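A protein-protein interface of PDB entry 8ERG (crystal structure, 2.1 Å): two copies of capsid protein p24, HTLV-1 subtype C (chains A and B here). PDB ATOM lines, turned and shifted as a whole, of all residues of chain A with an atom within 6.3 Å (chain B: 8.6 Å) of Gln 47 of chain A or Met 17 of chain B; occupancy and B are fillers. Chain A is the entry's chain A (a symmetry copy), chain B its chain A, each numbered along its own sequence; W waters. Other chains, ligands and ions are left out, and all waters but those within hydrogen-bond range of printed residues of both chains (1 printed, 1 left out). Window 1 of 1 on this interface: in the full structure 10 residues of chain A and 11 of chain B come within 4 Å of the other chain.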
ATOM      1  N   VAL A   2     -13.354 -33.896  -6.838  1.00  0.00           N
ATOM      2  CA  VAL A   2     -13.471 -34.858  -5.748  1.00  0.00           C
ATOM      3  C   VAL A   2     -14.055 -34.094  -4.564  1.00  0.00           C
ATOM      4  O   VAL A   2     -13.356 -33.336  -3.890  1.00  0.00           O
ATOM      5  CB  VAL A   2     -12.127 -35.504  -5.412  1.00  0.00           C
ATOM      6  CG1 VAL A   2     -12.283 -36.474  -4.249  1.00  0.00           C
ATOM      7  CG2 VAL A   2     -11.557 -36.216  -6.634  1.00  0.00           C
ATOM      8  N   ASP A  19     -18.894 -23.156 -12.227  1.00  0.00           N
ATOM      9  CA  ASP A  19     -17.506 -23.133 -11.777  1.00  0.00           C
ATOM     10  C   ASP A  19     -16.548 -22.987 -12.956  1.00  0.00           C
ATOM     11  O   ASP A  19     -15.591 -22.204 -12.898  1.00  0.00           O
ATOM     12  CB  ASP A  19     -17.204 -24.410 -10.996  1.00  0.00           C
ATOM     13  CG  ASP A  19     -17.978 -24.498  -9.685  1.00  0.00           C
ATOM     14  OD1 ASP A  19     -18.258 -23.444  -9.077  1.00  0.00           O
ATOM     15  OD2 ASP A  19     -18.296 -25.628  -9.260  1.00  0.00           O
ATOM     16  N   ALA A  22     -16.566 -19.424 -14.267  1.00  0.00           N
ATOM     17  CA  ALA A  22     -15.808 -18.503 -13.426  1.00  0.00           C
ATOM     18  C   ALA A  22     -14.313 -18.626 -13.688  1.00  0.00           C
ATOM     19  O   ALA A  22     -13.587 -17.625 -13.669  1.00  0.00           O
ATOM     20  CB  ALA A  22     -16.117 -18.764 -11.951  1.00  0.00           C
ATOM     21  N   ILE A  23     -13.833 -19.846 -13.934  1.00  0.00           N
ATOM     22  CA  ILE A  23     -12.417 -20.042 -14.224  1.00  0.00           C
ATOM     23  C   ILE A  23     -12.061 -19.427 -15.573  1.00  0.00           C
ATOM     24  O   ILE A  23     -11.051 -18.727 -15.708  1.00  0.00           O
ATOM     25  CB  ILE A  23     -12.067 -21.541 -14.187  1.00  0.00           C
ATOM     26  CG1 ILE A  23     -12.159 -22.078 -12.757  1.00  0.00           C
ATOM     27  CG2 ILE A  23     -10.672 -21.771 -14.748  1.00  0.00           C
ATOM     28  CD1 ILE A  23     -12.327 -23.577 -12.676  1.00  0.00           C
ATOM     29  N   LYS A  24     -12.884 -19.683 -16.593  1.00  0.00           N
ATOM     30  CA  LYS A  24     -12.559 -19.212 -17.934  1.00  0.00           C
ATOM     31  C   LYS A  24     -12.507 -17.692 -17.993  1.00  0.00           C
ATOM     32  O   LYS A  24     -11.623 -17.118 -18.638  1.00  0.00           O
ATOM     33  CB  LYS A  24     -13.575 -19.746 -18.943  1.00  0.00           C
ATOM     34  CG  LYS A  24     -13.084 -19.696 -20.384  1.00  0.00           C
ATOM     35  CD  LYS A  24     -13.924 -20.576 -21.293  1.00  0.00           C
ATOM     36  CE  LYS A  24     -13.151 -21.017 -22.526  1.00  0.00           C
ATOM     37  NZ  LYS A  24     -13.902 -22.044 -23.306  1.00  0.00           N
ATOM     38  N   GLU A  26     -11.791 -15.664 -15.611  1.00  0.00           N
ATOM     39  CA  GLU A  26     -10.629 -15.151 -14.898  1.00  0.00           C
ATOM     40  C   GLU A  26      -9.378 -15.207 -15.765  1.00  0.00           C
ATOM     41  O   GLU A  26      -8.463 -14.395 -15.582  1.00  0.00           O
ATOM     42  CB  GLU A  26     -10.418 -15.937 -13.606  1.00  0.00           C
ATOM     43  CG  GLU A  26      -9.450 -15.274 -12.640  1.00  0.00           C
ATOM     44  CD  GLU A  26      -9.703 -15.664 -11.200  1.00  0.00           C
ATOM     45  OE1 GLU A  26     -10.440 -16.645 -10.966  1.00  0.00           O
ATOM     46  OE2 GLU A  26      -9.161 -14.990 -10.299  1.00  0.00           O
ATOM     47  N   THR A  40      -4.513 -18.902 -11.574  1.00  0.00           N
ATOM     48  CA  THR A  40      -5.939 -19.206 -11.526  1.00  0.00           C
ATOM     49  C   THR A  40      -6.180 -20.709 -11.440  1.00  0.00           C
ATOM     50  O   THR A  40      -6.979 -21.171 -10.617  1.00  0.00           O
ATOM     51  CB  THR A  40      -6.643 -18.621 -12.752  1.00  0.00           C
ATOM     52  OG1 THR A  40      -6.522 -17.193 -12.743  1.00  0.00           O
ATOM     53  CG2 THR A  40      -8.120 -19.000 -12.756  1.00  0.00           C
ATOM     54  N   ARG A  42      -4.128 -23.012 -10.469  1.00  0.00           N
ATOM     55  CA  ARG A  42      -3.602 -23.558  -9.222  1.00  0.00           C
ATOM     56  C   ARG A  42      -4.638 -23.456  -8.109  1.00  0.00           C
ATOM     57  O   ARG A  42      -4.801 -24.388  -7.314  1.00  0.00           O
ATOM     58  CB  ARG A  42      -2.309 -22.840  -8.838  1.00  0.00           C
ATOM     59  CG  ARG A  42      -1.061 -23.485  -9.435  1.00  0.00           C
ATOM     60  CD  ARG A  42       0.218 -22.787  -8.990  1.00  0.00           C
ATOM     61  NE  ARG A  42       1.349 -23.146  -9.839  1.00  0.00           N
ATOM     62  CZ  ARG A  42       2.044 -24.271  -9.729  1.00  0.00           C
ATOM     63  NH1 ARG A  42       1.765 -25.170  -8.800  1.00  0.00           N
ATOM     64  NH2 ARG A  42       3.045 -24.499 -10.575  1.00  0.00           N
ATOM     65  N   LEU A  43      -5.366 -22.338  -8.049  1.00  0.00           N
ATOM     66  CA  LEU A  43      -6.413 -22.202  -7.043  1.00  0.00           C
ATOM     67  C   LEU A  43      -7.620 -23.075  -7.372  1.00  0.00           C
ATOM     68  O   LEU A  43      -8.276 -23.590  -6.460  1.00  0.00           O
ATOM     69  CB  LEU A  43      -6.831 -20.740  -6.918  1.00  0.00           C
ATOM     70  CG  LEU A  43      -5.739 -19.790  -6.420  1.00  0.00           C
ATOM     71  CD1 LEU A  43      -6.076 -18.359  -6.792  1.00  0.00           C
ATOM     72  CD2 LEU A  43      -5.545 -19.922  -4.918  1.00  0.00           C
ATOM     73  N   ALA A  44      -7.925 -23.254  -8.659  1.00  0.00           N
ATOM     74  CA  ALA A  44      -9.027 -24.130  -9.042  1.00  0.00           C
ATOM     75  C   ALA A  44      -8.711 -25.585  -8.716  1.00  0.00           C
ATOM     76  O   ALA A  44      -9.589 -26.335  -8.271  1.00  0.00           O
ATOM     77  CB  ALA A  44      -9.334 -23.971 -10.530  1.00  0.00           C
ATOM     78  N   VAL A  45      -7.464 -26.006  -8.940  1.00  0.00           N
ATOM     79  CA  VAL A  45      -7.060 -27.355  -8.558  1.00  0.00           C
ATOM     80  C   VAL A  45      -7.170 -27.532  -7.050  1.00  0.00           C
ATOM     81  O   VAL A  45      -7.615 -28.577  -6.559  1.00  0.00           O
ATOM     82  CB  VAL A  45      -5.631 -27.643  -9.059  1.00  0.00           C
ATOM     83  CG1 VAL A  45      -5.048 -28.865  -8.357  1.00  0.00           C
ATOM     84  CG2 VAL A  45      -5.628 -27.833 -10.568  1.00  0.00           C
ATOM     85  N   GLN A  46      -6.772 -26.509  -6.293  1.00  0.00           N
ATOM     86  CA  GLN A  46      -6.849 -26.575  -4.838  1.00  0.00           C
ATOM     87  C   GLN A  46      -8.293 -26.650  -4.361  1.00  0.00           C
ATOM     88  O   GLN A  46      -8.610 -27.398  -3.428  1.00  0.00           O
ATOM     89  CB  GLN A  46      -6.150 -25.357  -4.241  1.00  0.00           C
ATOM     90  CG  GLN A  46      -5.828 -25.460  -2.766  1.00  0.00           C
ATOM     91  CD  GLN A  46      -4.996 -24.293  -2.288  1.00  0.00           C
ATOM     92  OE1 GLN A  46      -3.844 -24.459  -1.890  1.00  0.00           O
ATOM     93  NE2 GLN A  46      -5.571 -23.096  -2.335  1.00  0.00           N
ATOM     94  N   GLN A  47      -9.185 -25.886  -4.990  1.00  0.00           N
ATOM     95  CA  GLN A  47     -10.565 -25.826  -4.528  1.00  0.00           C
ATOM     96  C   GLN A  47     -11.330 -27.099  -4.872  1.00  0.00           C
ATOM     97  O   GLN A  47     -12.088 -27.617  -4.044  1.00  0.00           O
ATOM     98  CB  GLN A  47     -11.262 -24.610  -5.140  1.00  0.00           C
ATOM     99  CG  GLN A  47     -12.784 -24.668  -5.083  1.00  0.00           C
ATOM    100  CD  GLN A  47     -13.440 -23.383  -5.562  1.00  0.00           C
ATOM    101  OE1 GLN A  47     -12.788 -22.521  -6.142  1.00  0.00           O
ATOM    102  NE2 GLN A  47     -14.738 -23.254  -5.319  1.00  0.00           N
ATOM    103  N   PHE A  48     -11.163 -27.609  -6.089  1.00  0.00           N
ATOM    104  CA  PHE A  48     -12.012 -28.684  -6.582  1.00  0.00           C
ATOM    105  C   PHE A  48     -11.363 -30.059  -6.516  1.00  0.00           C
ATOM    106  O   PHE A  48     -12.057 -31.057  -6.733  1.00  0.00           O
ATOM    107  CB  PHE A  48     -12.442 -28.379  -8.021  1.00  0.00           C
ATOM    108  CG  PHE A  48     -13.293 -27.147  -8.140  1.00  0.00           C
ATOM    109  CD1 PHE A  48     -14.620 -27.168  -7.741  1.00  0.00           C
ATOM    110  CD2 PHE A  48     -12.764 -25.964  -8.623  1.00  0.00           C
ATOM    111  CE1 PHE A  48     -15.407 -26.034  -7.837  1.00  0.00           C
ATOM    112  CE2 PHE A  48     -13.545 -24.827  -8.723  1.00  0.00           C
ATOM    113  CZ  PHE A  48     -14.870 -24.863  -8.327  1.00  0.00           C
ATOM    114  N   ASP A  49     -10.070 -30.138  -6.209  1.00  0.00           N
ATOM    115  CA  ASP A  49      -9.362 -31.406  -6.071  1.00  0.00           C
ATOM    116  C   ASP A  49      -9.685 -32.338  -7.243  1.00  0.00           C
ATOM    117  O   ASP A  49     -10.216 -33.433  -7.047  1.00  0.00           O
ATOM    118  CB  ASP A  49      -9.705 -32.068  -4.743  1.00  0.00           C
ATOM    119  CG  ASP A  49      -8.661 -33.078  -4.303  1.00  0.00           C
ATOM    120  OD1 ASP A  49      -7.665 -33.273  -5.032  1.00  0.00           O
ATOM    121  OD2 ASP A  49      -8.837 -33.678  -3.222  1.00  0.00           O
ATOM    122  N   PRO A  50      -9.378 -31.928  -8.471  1.00  0.00           N
ATOM    123  CA  PRO A  50      -9.837 -32.691  -9.636  1.00  0.00           C
ATOM    124  C   PRO A  50      -9.046 -33.972  -9.851  1.00  0.00           C
ATOM    125  O   PRO A  50      -7.859 -34.067  -9.535  1.00  0.00           O
ATOM    126  CB  PRO A  50      -9.627 -31.713 -10.799  1.00  0.00           C
ATOM    127  CG  PRO A  50      -8.494 -30.839 -10.347  1.00  0.00           C
ATOM    128  CD  PRO A  50      -8.644 -30.708  -8.853  1.00  0.00           C
ATOM    129  N   ARG B  13     -11.071 -25.527   5.097  1.00  0.00           N
ATOM    130  CA  ARG B  13     -11.616 -25.754   3.774  1.00  0.00           C
ATOM    131  C   ARG B  13     -10.919 -24.782   2.831  1.00  0.00           C
ATOM    132  O   ARG B  13     -10.697 -23.617   3.197  1.00  0.00           O
ATOM    133  CB  ARG B  13     -13.135 -25.549   3.746  1.00  0.00           C
ATOM    134  CG  ARG B  13     -13.922 -26.836   3.524  1.00  0.00           C
ATOM    135  CD  ARG B  13     -14.104 -27.667   4.795  1.00  0.00           C
ATOM    136  NE  ARG B  13     -14.999 -28.790   4.534  1.00  0.00           N
ATOM    137  CZ  ARG B  13     -14.694 -30.072   4.699  1.00  0.00           C
ATOM    138  NH1 ARG B  13     -13.558 -30.450   5.264  1.00  0.00           N
ATOM    139  NH2 ARG B  13     -15.555 -30.999   4.289  1.00  0.00           N
ATOM    140  N   PRO B  14     -10.546 -25.220   1.631  1.00  0.00           N
ATOM    141  CA  PRO B  14      -9.731 -24.367   0.757  1.00  0.00           C
ATOM    142  C   PRO B  14     -10.491 -23.124   0.317  1.00  0.00           C
ATOM    143  O   PRO B  14     -11.708 -23.005   0.472  1.00  0.00           O
ATOM    144  CB  PRO B  14      -9.404 -25.277  -0.431  1.00  0.00           C
ATOM    145  CG  PRO B  14     -10.517 -26.267  -0.461  1.00  0.00           C
ATOM    146  CD  PRO B  14     -10.900 -26.495   0.978  1.00  0.00           C
ATOM    147  N   TRP B  15      -9.735 -22.178  -0.237  1.00  0.00           N
ATOM    148  CA  TRP B  15     -10.334 -20.966  -0.776  1.00  0.00           C
ATOM    149  C   TRP B  15     -11.329 -21.312  -1.878  1.00  0.00           C
ATOM    150  O   TRP B  15     -11.090 -22.206  -2.695  1.00  0.00           O
ATOM    151  CB  TRP B  15      -9.251 -20.040  -1.331  1.00  0.00           C
ATOM    152  CG  TRP B  15      -8.520 -19.244  -0.293  1.00  0.00           C
ATOM    153  CD1 TRP B  15      -7.201 -19.347   0.039  1.00  0.00           C
ATOM    154  CD2 TRP B  15      -9.063 -18.211   0.539  1.00  0.00           C
ATOM    155  NE1 TRP B  15      -6.889 -18.448   1.031  1.00  0.00           N
ATOM    156  CE2 TRP B  15      -8.015 -17.739   1.355  1.00  0.00           C
ATOM    157  CE3 TRP B  15     -10.332 -17.644   0.677  1.00  0.00           C
ATOM    158  CZ2 TRP B  15      -8.198 -16.726   2.292  1.00  0.00           C
ATOM    159  CZ3 TRP B  15     -10.511 -16.640   1.609  1.00  0.00           C
ATOM    160  CH2 TRP B  15      -9.450 -16.192   2.403  1.00  0.00           C
ATOM    161  N   GLN B  16     -12.452 -20.601  -1.894  1.00  0.00           N
ATOM    162  CA  GLN B  16     -13.442 -20.717  -2.955  1.00  0.00           C
ATOM    163  C   GLN B  16     -13.203 -19.602  -3.966  1.00  0.00           C
ATOM    164  O   GLN B  16     -13.048 -18.437  -3.586  1.00  0.00           O
ATOM    165  CB  GLN B  16     -14.866 -20.634  -2.401  1.00  0.00           C
ATOM    166  CG  GLN B  16     -15.131 -21.545  -1.209  1.00  0.00           C
ATOM    167  CD  GLN B  16     -15.466 -22.964  -1.617  1.00  0.00           C
ATOM    168  OE1 GLN B  16     -16.515 -23.220  -2.209  1.00  0.00           O
ATOM    169  NE2 GLN B  16     -14.576 -23.897  -1.302  1.00  0.00           N
ATOM    170  N   MET B  17     -13.176 -19.961  -5.250  1.00  0.00           N
ATOM    171  CA  MET B  17     -12.845 -18.977  -6.274  1.00  0.00           C
ATOM    172  C   MET B  17     -13.831 -17.815  -6.268  1.00  0.00           C
ATOM    173  O   MET B  17     -13.443 -16.664  -6.497  1.00  0.00           O
ATOM    174  CB  MET B  17     -12.804 -19.640  -7.648  1.00  0.00           C
ATOM    175  CG  MET B  17     -11.536 -20.454  -7.887  1.00  0.00           C
ATOM    176  SD  MET B  17     -11.442 -21.159  -9.540  1.00  0.00           S
ATOM    177  CE  MET B  17     -11.387 -19.664 -10.521  1.00  0.00           C
ATOM    178  N   LYS B  18     -15.110 -18.092  -6.001  1.00  0.00           N
ATOM    179  CA  LYS B  18     -16.093 -17.016  -5.950  1.00  0.00           C
ATOM    180  C   LYS B  18     -15.798 -16.036  -4.820  1.00  0.00           C
ATOM    181  O   LYS B  18     -16.081 -14.839  -4.949  1.00  0.00           O
ATOM    182  CB  LYS B  18     -17.497 -17.602  -5.805  1.00  0.00           C
ATOM    183  CG  LYS B  18     -17.969 -18.353  -7.041  1.00  0.00           C
ATOM    184  CD  LYS B  18     -19.375 -18.908  -6.873  1.00  0.00           C
ATOM    185  CE  LYS B  18     -19.826 -19.633  -8.132  1.00  0.00           C
ATOM    186  NZ  LYS B  18     -21.192 -20.207  -8.001  1.00  0.00           N
ATOM    187  N   ASP B  19     -15.236 -16.519  -3.711  1.00  0.00           N
ATOM    188  CA  ASP B  19     -14.835 -15.629  -2.626  1.00  0.00           C
ATOM    189  C   ASP B  19     -13.583 -14.838  -2.996  1.00  0.00           C
ATOM    190  O   ASP B  19     -13.508 -13.627  -2.753  1.00  0.00           O
ATOM    191  CB  ASP B  19     -14.594 -16.449  -1.359  1.00  0.00           C
ATOM    192  CG  ASP B  19     -15.869 -17.084  -0.817  1.00  0.00           C
ATOM    193  OD1 ASP B  19     -16.956 -16.494  -0.982  1.00  0.00           O
ATOM    194  OD2 ASP B  19     -15.777 -18.173  -0.213  1.00  0.00           O
ATOM    195  N   LEU B  20     -12.592 -15.514  -3.586  1.00  0.00           N
ATOM    196  CA  LEU B  20     -11.378 -14.838  -4.029  1.00  0.00           C
ATOM    197  C   LEU B  20     -11.698 -13.773  -5.072  1.00  0.00           C
ATOM    198  O   LEU B  20     -11.170 -12.655  -5.010  1.00  0.00           O
ATOM    199  CB  LEU B  20     -10.386 -15.867  -4.578  1.00  0.00           C
ATOM    200  CG  LEU B  20      -9.703 -16.758  -3.534  1.00  0.00           C
ATOM    201  CD1 LEU B  20      -8.710 -17.699  -4.195  1.00  0.00           C
ATOM    202  CD2 LEU B  20      -9.007 -15.926  -2.469  1.00  0.00           C
ATOM    203  N   GLN B  21     -12.589 -14.086  -6.015  1.00  0.00           N
ATOM    204  CA  GLN B  21     -12.928 -13.125  -7.062  1.00  0.00           C
ATOM    205  C   GLN B  21     -13.597 -11.886  -6.478  1.00  0.00           C
ATOM    206  O   GLN B  21     -13.362 -10.766  -6.946  1.00  0.00           O
ATOM    207  CB  GLN B  21     -13.830 -13.783  -8.106  1.00  0.00           C
ATOM    208  CG  GLN B  21     -13.077 -14.595  -9.147  1.00  0.00           C
ATOM    209  CD  GLN B  21     -13.995 -15.450  -9.997  1.00  0.00           C
ATOM    210  OE1 GLN B  21     -15.218 -15.375  -9.876  1.00  0.00           O
ATOM    211  NE2 GLN B  21     -13.409 -16.269 -10.862  1.00  0.00           N
ATOM    212  N   ALA B  22     -14.428 -12.065  -5.449  1.00  0.00           N
ATOM    213  CA  ALA B  22     -15.069 -10.919  -4.815  1.00  0.00           C
ATOM    214  C   ALA B  22     -14.045 -10.034  -4.117  1.00  0.00           C
ATOM    215  O   ALA B  22     -14.171  -8.803  -4.122  1.00  0.00           O
ATOM    216  CB  ALA B  22     -16.132 -11.394  -3.822  1.00  0.00           C
ATOM    217  N   ILE B  23     -13.024 -10.641  -3.511  1.00  0.00           N
ATOM    218  CA  ILE B  23     -11.985  -9.861  -2.847  1.00  0.00           C
ATOM    219  C   ILE B  23     -11.161  -9.092  -3.873  1.00  0.00           C
ATOM    220  O   ILE B  23     -10.883  -7.899  -3.702  1.00  0.00           O
ATOM    221  CB  ILE B  23     -11.093 -10.779  -1.992  1.00  0.00           C
ATOM    222  CG1 ILE B  23     -11.874 -11.323  -0.794  1.00  0.00           C
ATOM    223  CG2 ILE B  23      -9.860 -10.026  -1.519  1.00  0.00           C
ATOM    224  CD1 ILE B  23     -11.282 -12.579  -0.196  1.00  0.00           C
ATOM    225  N   LYS B  24     -10.755  -9.764  -4.952  1.00  0.00           N
ATOM    226  CA  LYS B  24      -9.881  -9.125  -5.929  1.00  0.00           C
ATOM    227  C   LYS B  24     -10.559  -7.930  -6.585  1.00  0.00           C
ATOM    228  O   LYS B  24      -9.929  -6.887  -6.795  1.00  0.00           O
ATOM    229  CB  LYS B  24      -9.447 -10.134  -6.991  1.00  0.00           C
ATOM    230  CG  LYS B  24      -8.210  -9.703  -7.769  1.00  0.00           C
ATOM    231  CD  LYS B  24      -7.584 -10.868  -8.516  1.00  0.00           C
ATOM    232  CE  LYS B  24      -6.104 -10.641  -8.781  1.00  0.00           C
ATOM    233  NZ  LYS B  24      -5.449 -11.867  -9.323  1.00  0.00           N
ATOM    234  N   ASP B  57      -1.607 -18.211   0.260  1.00  0.00           N
ATOM    235  CA  ASP B  57      -2.286 -18.291  -1.030  1.00  0.00           C
ATOM    236  C   ASP B  57      -2.959 -16.971  -1.388  1.00  0.00           C
ATOM    237  O   ASP B  57      -2.910 -16.537  -2.545  1.00  0.00           O
ATOM    238  CB  ASP B  57      -3.313 -19.425  -1.010  1.00  0.00           C
ATOM    239  CG  ASP B  57      -2.672 -20.790  -0.885  1.00  0.00           C
ATOM    240  OD1 ASP B  57      -1.448 -20.897  -1.107  1.00  0.00           O
ATOM    241  OD2 ASP B  57      -3.392 -21.757  -0.559  1.00  0.00           O
ATOM    242  N   TYR B  61      -2.375 -14.508  -4.736  1.00  0.00           N
ATOM    243  CA  TYR B  61      -3.466 -14.261  -5.671  1.00  0.00           C
ATOM    244  C   TYR B  61      -3.683 -12.773  -5.913  1.00  0.00           C
ATOM    245  O   TYR B  61      -4.054 -12.378  -7.024  1.00  0.00           O
ATOM    246  CB  TYR B  61      -4.748 -14.903  -5.143  1.00  0.00           C
ATOM    247  CG  TYR B  61      -5.971 -14.658  -5.996  1.00  0.00           C
ATOM    248  CD1 TYR B  61      -6.075 -15.203  -7.269  1.00  0.00           C
ATOM    249  CD2 TYR B  61      -7.025 -13.893  -5.523  1.00  0.00           C
ATOM    250  CE1 TYR B  61      -7.194 -14.988  -8.049  1.00  0.00           C
ATOM    251  CE2 TYR B  61      -8.146 -13.671  -6.294  1.00  0.00           C
ATOM    252  CZ  TYR B  61      -8.229 -14.223  -7.555  1.00  0.00           C
ATOM    253  OH  TYR B  61      -9.347 -14.000  -8.323  1.00  0.00           O
HETATM  254  O   HOH W   1     -14.539 -21.950 -10.241  1.00  0.00           O
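NE2 of Gln 16 of chain B lies within hydrogen-bond range of O of Pro 14 of chain B, at 3.5 Å.
The side-chain amino group (NZ) of Lys 24 of chain B lies within hydrogen-bond range of the backbone carbonyl oxygen (O) of Tyr 61 of chain B (2.7 Å).
Of chain B, only Trp 15, Gln 16 and Met 17 come within 4 Å of Gln 47 of chain A.
Printed residues of chain A within 4 Å of Met 17 of chain B: Ile 23 (3.4 Å), Glu 26 (3.2 Å), Ala 44 (3.7 Å) and Gln 47 (2.7 Å).
No residue of chain B comes within 4 Å of Phe 48 of chain A.
Printed residues of chain B within 4 Å of Gln 46 of chain A: Pro 14 (3.7 Å) and Asp 57 (3.0 Å).
Of the printed residues of chain A, Gln 21 of chain B touches Ala 22 (3.1 Å) and Glu 26 (3.0 Å).
Of the printed residues of chain A, Tyr 61 of chain B touches Glu 26 and Leu 43.
Of the printed residues of chain A, Trp 15 of chain B touches Gln 47 (3.4 Å).
Of the printed residues of chain A, Pro 14 of chain B touches Gln 46 (3.7 Å).
The nearest residue of chain B that does not touch Gln 47 of chain A is Pro 14 of chain B (4.1 Å).
The nearest printed residue of chain A that does not touch Met 17 of chain B is Thr 40 of chain A (4.01 Å).
The nearest printed residue of chain A that does not touch Asp 57 of chain B is Leu 43 of chain A (4.5 Å).
NE2 of Gln 21 of chain B lies within hydrogen-bond range of O of Ala 22 of chain A (3.1 Å).
OE2 of Glu 26 of chain A sits close to OH of Tyr 61 of chain B.
The side-chain carboxylate (OD2) of Asp 57 of chain B lies close to the side-chain amide oxygen (OE1) of Gln 46 of chain A (3.0 Å).
N of Met 17 of chain B is in hydrogen-bond range of OE1 of Gln 47 of chain A (2.7 Å).
The side-chain carboxylate (OE1) of Glu 26 of chain A lies within hydrogen-bond range of the side-chain amide nitrogen (NE2) of Gln 21 of chain B (3.0 Å).
Among the printed residues, pairs that only touch across the chains: Leu 43 of chain A with Tyr 61 of chain B (3.2 Å), Glu 26 of chain A with Met 17 of chain B (3.2 Å), Ile 23 of chain A with Met 17 of chain B (3.4 Å), Gln 47 of chain A with Trp 15 of chain B (3.4 Å), Gln 47 of chain A with Gln 16 of chain B (3.6 Å), Ala 44 of chain A with Met 17 of chain B (3.7 Å), Gln 46 of chain A with Pro 14 of chain B (3.7 Å) and Leu 43 of chain A with Leu 20 of chain B (3.8 Å).
Water W1 lies within hydrogen-bond range of O of Asp 19 of chain A and SD of Met 17 of chain B.
4 positions are printed for both chains.
Of the 14 printed residues of chain B, 8 touch a printed residue of chain A.
Hydrophobic or aromatic side chains of chain B within 4 Å of the printed part of chain A: Pro 14, Met 17, Leu 20 and Tyr 61.
Along chain A the printed residues that touch a printed residue of chain B span positions 22 to 47.
Among the printed residues, no Asp or Glu carboxylate lies within 4 Å of a Lys or Arg side-chain nitrogen of the other chain.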
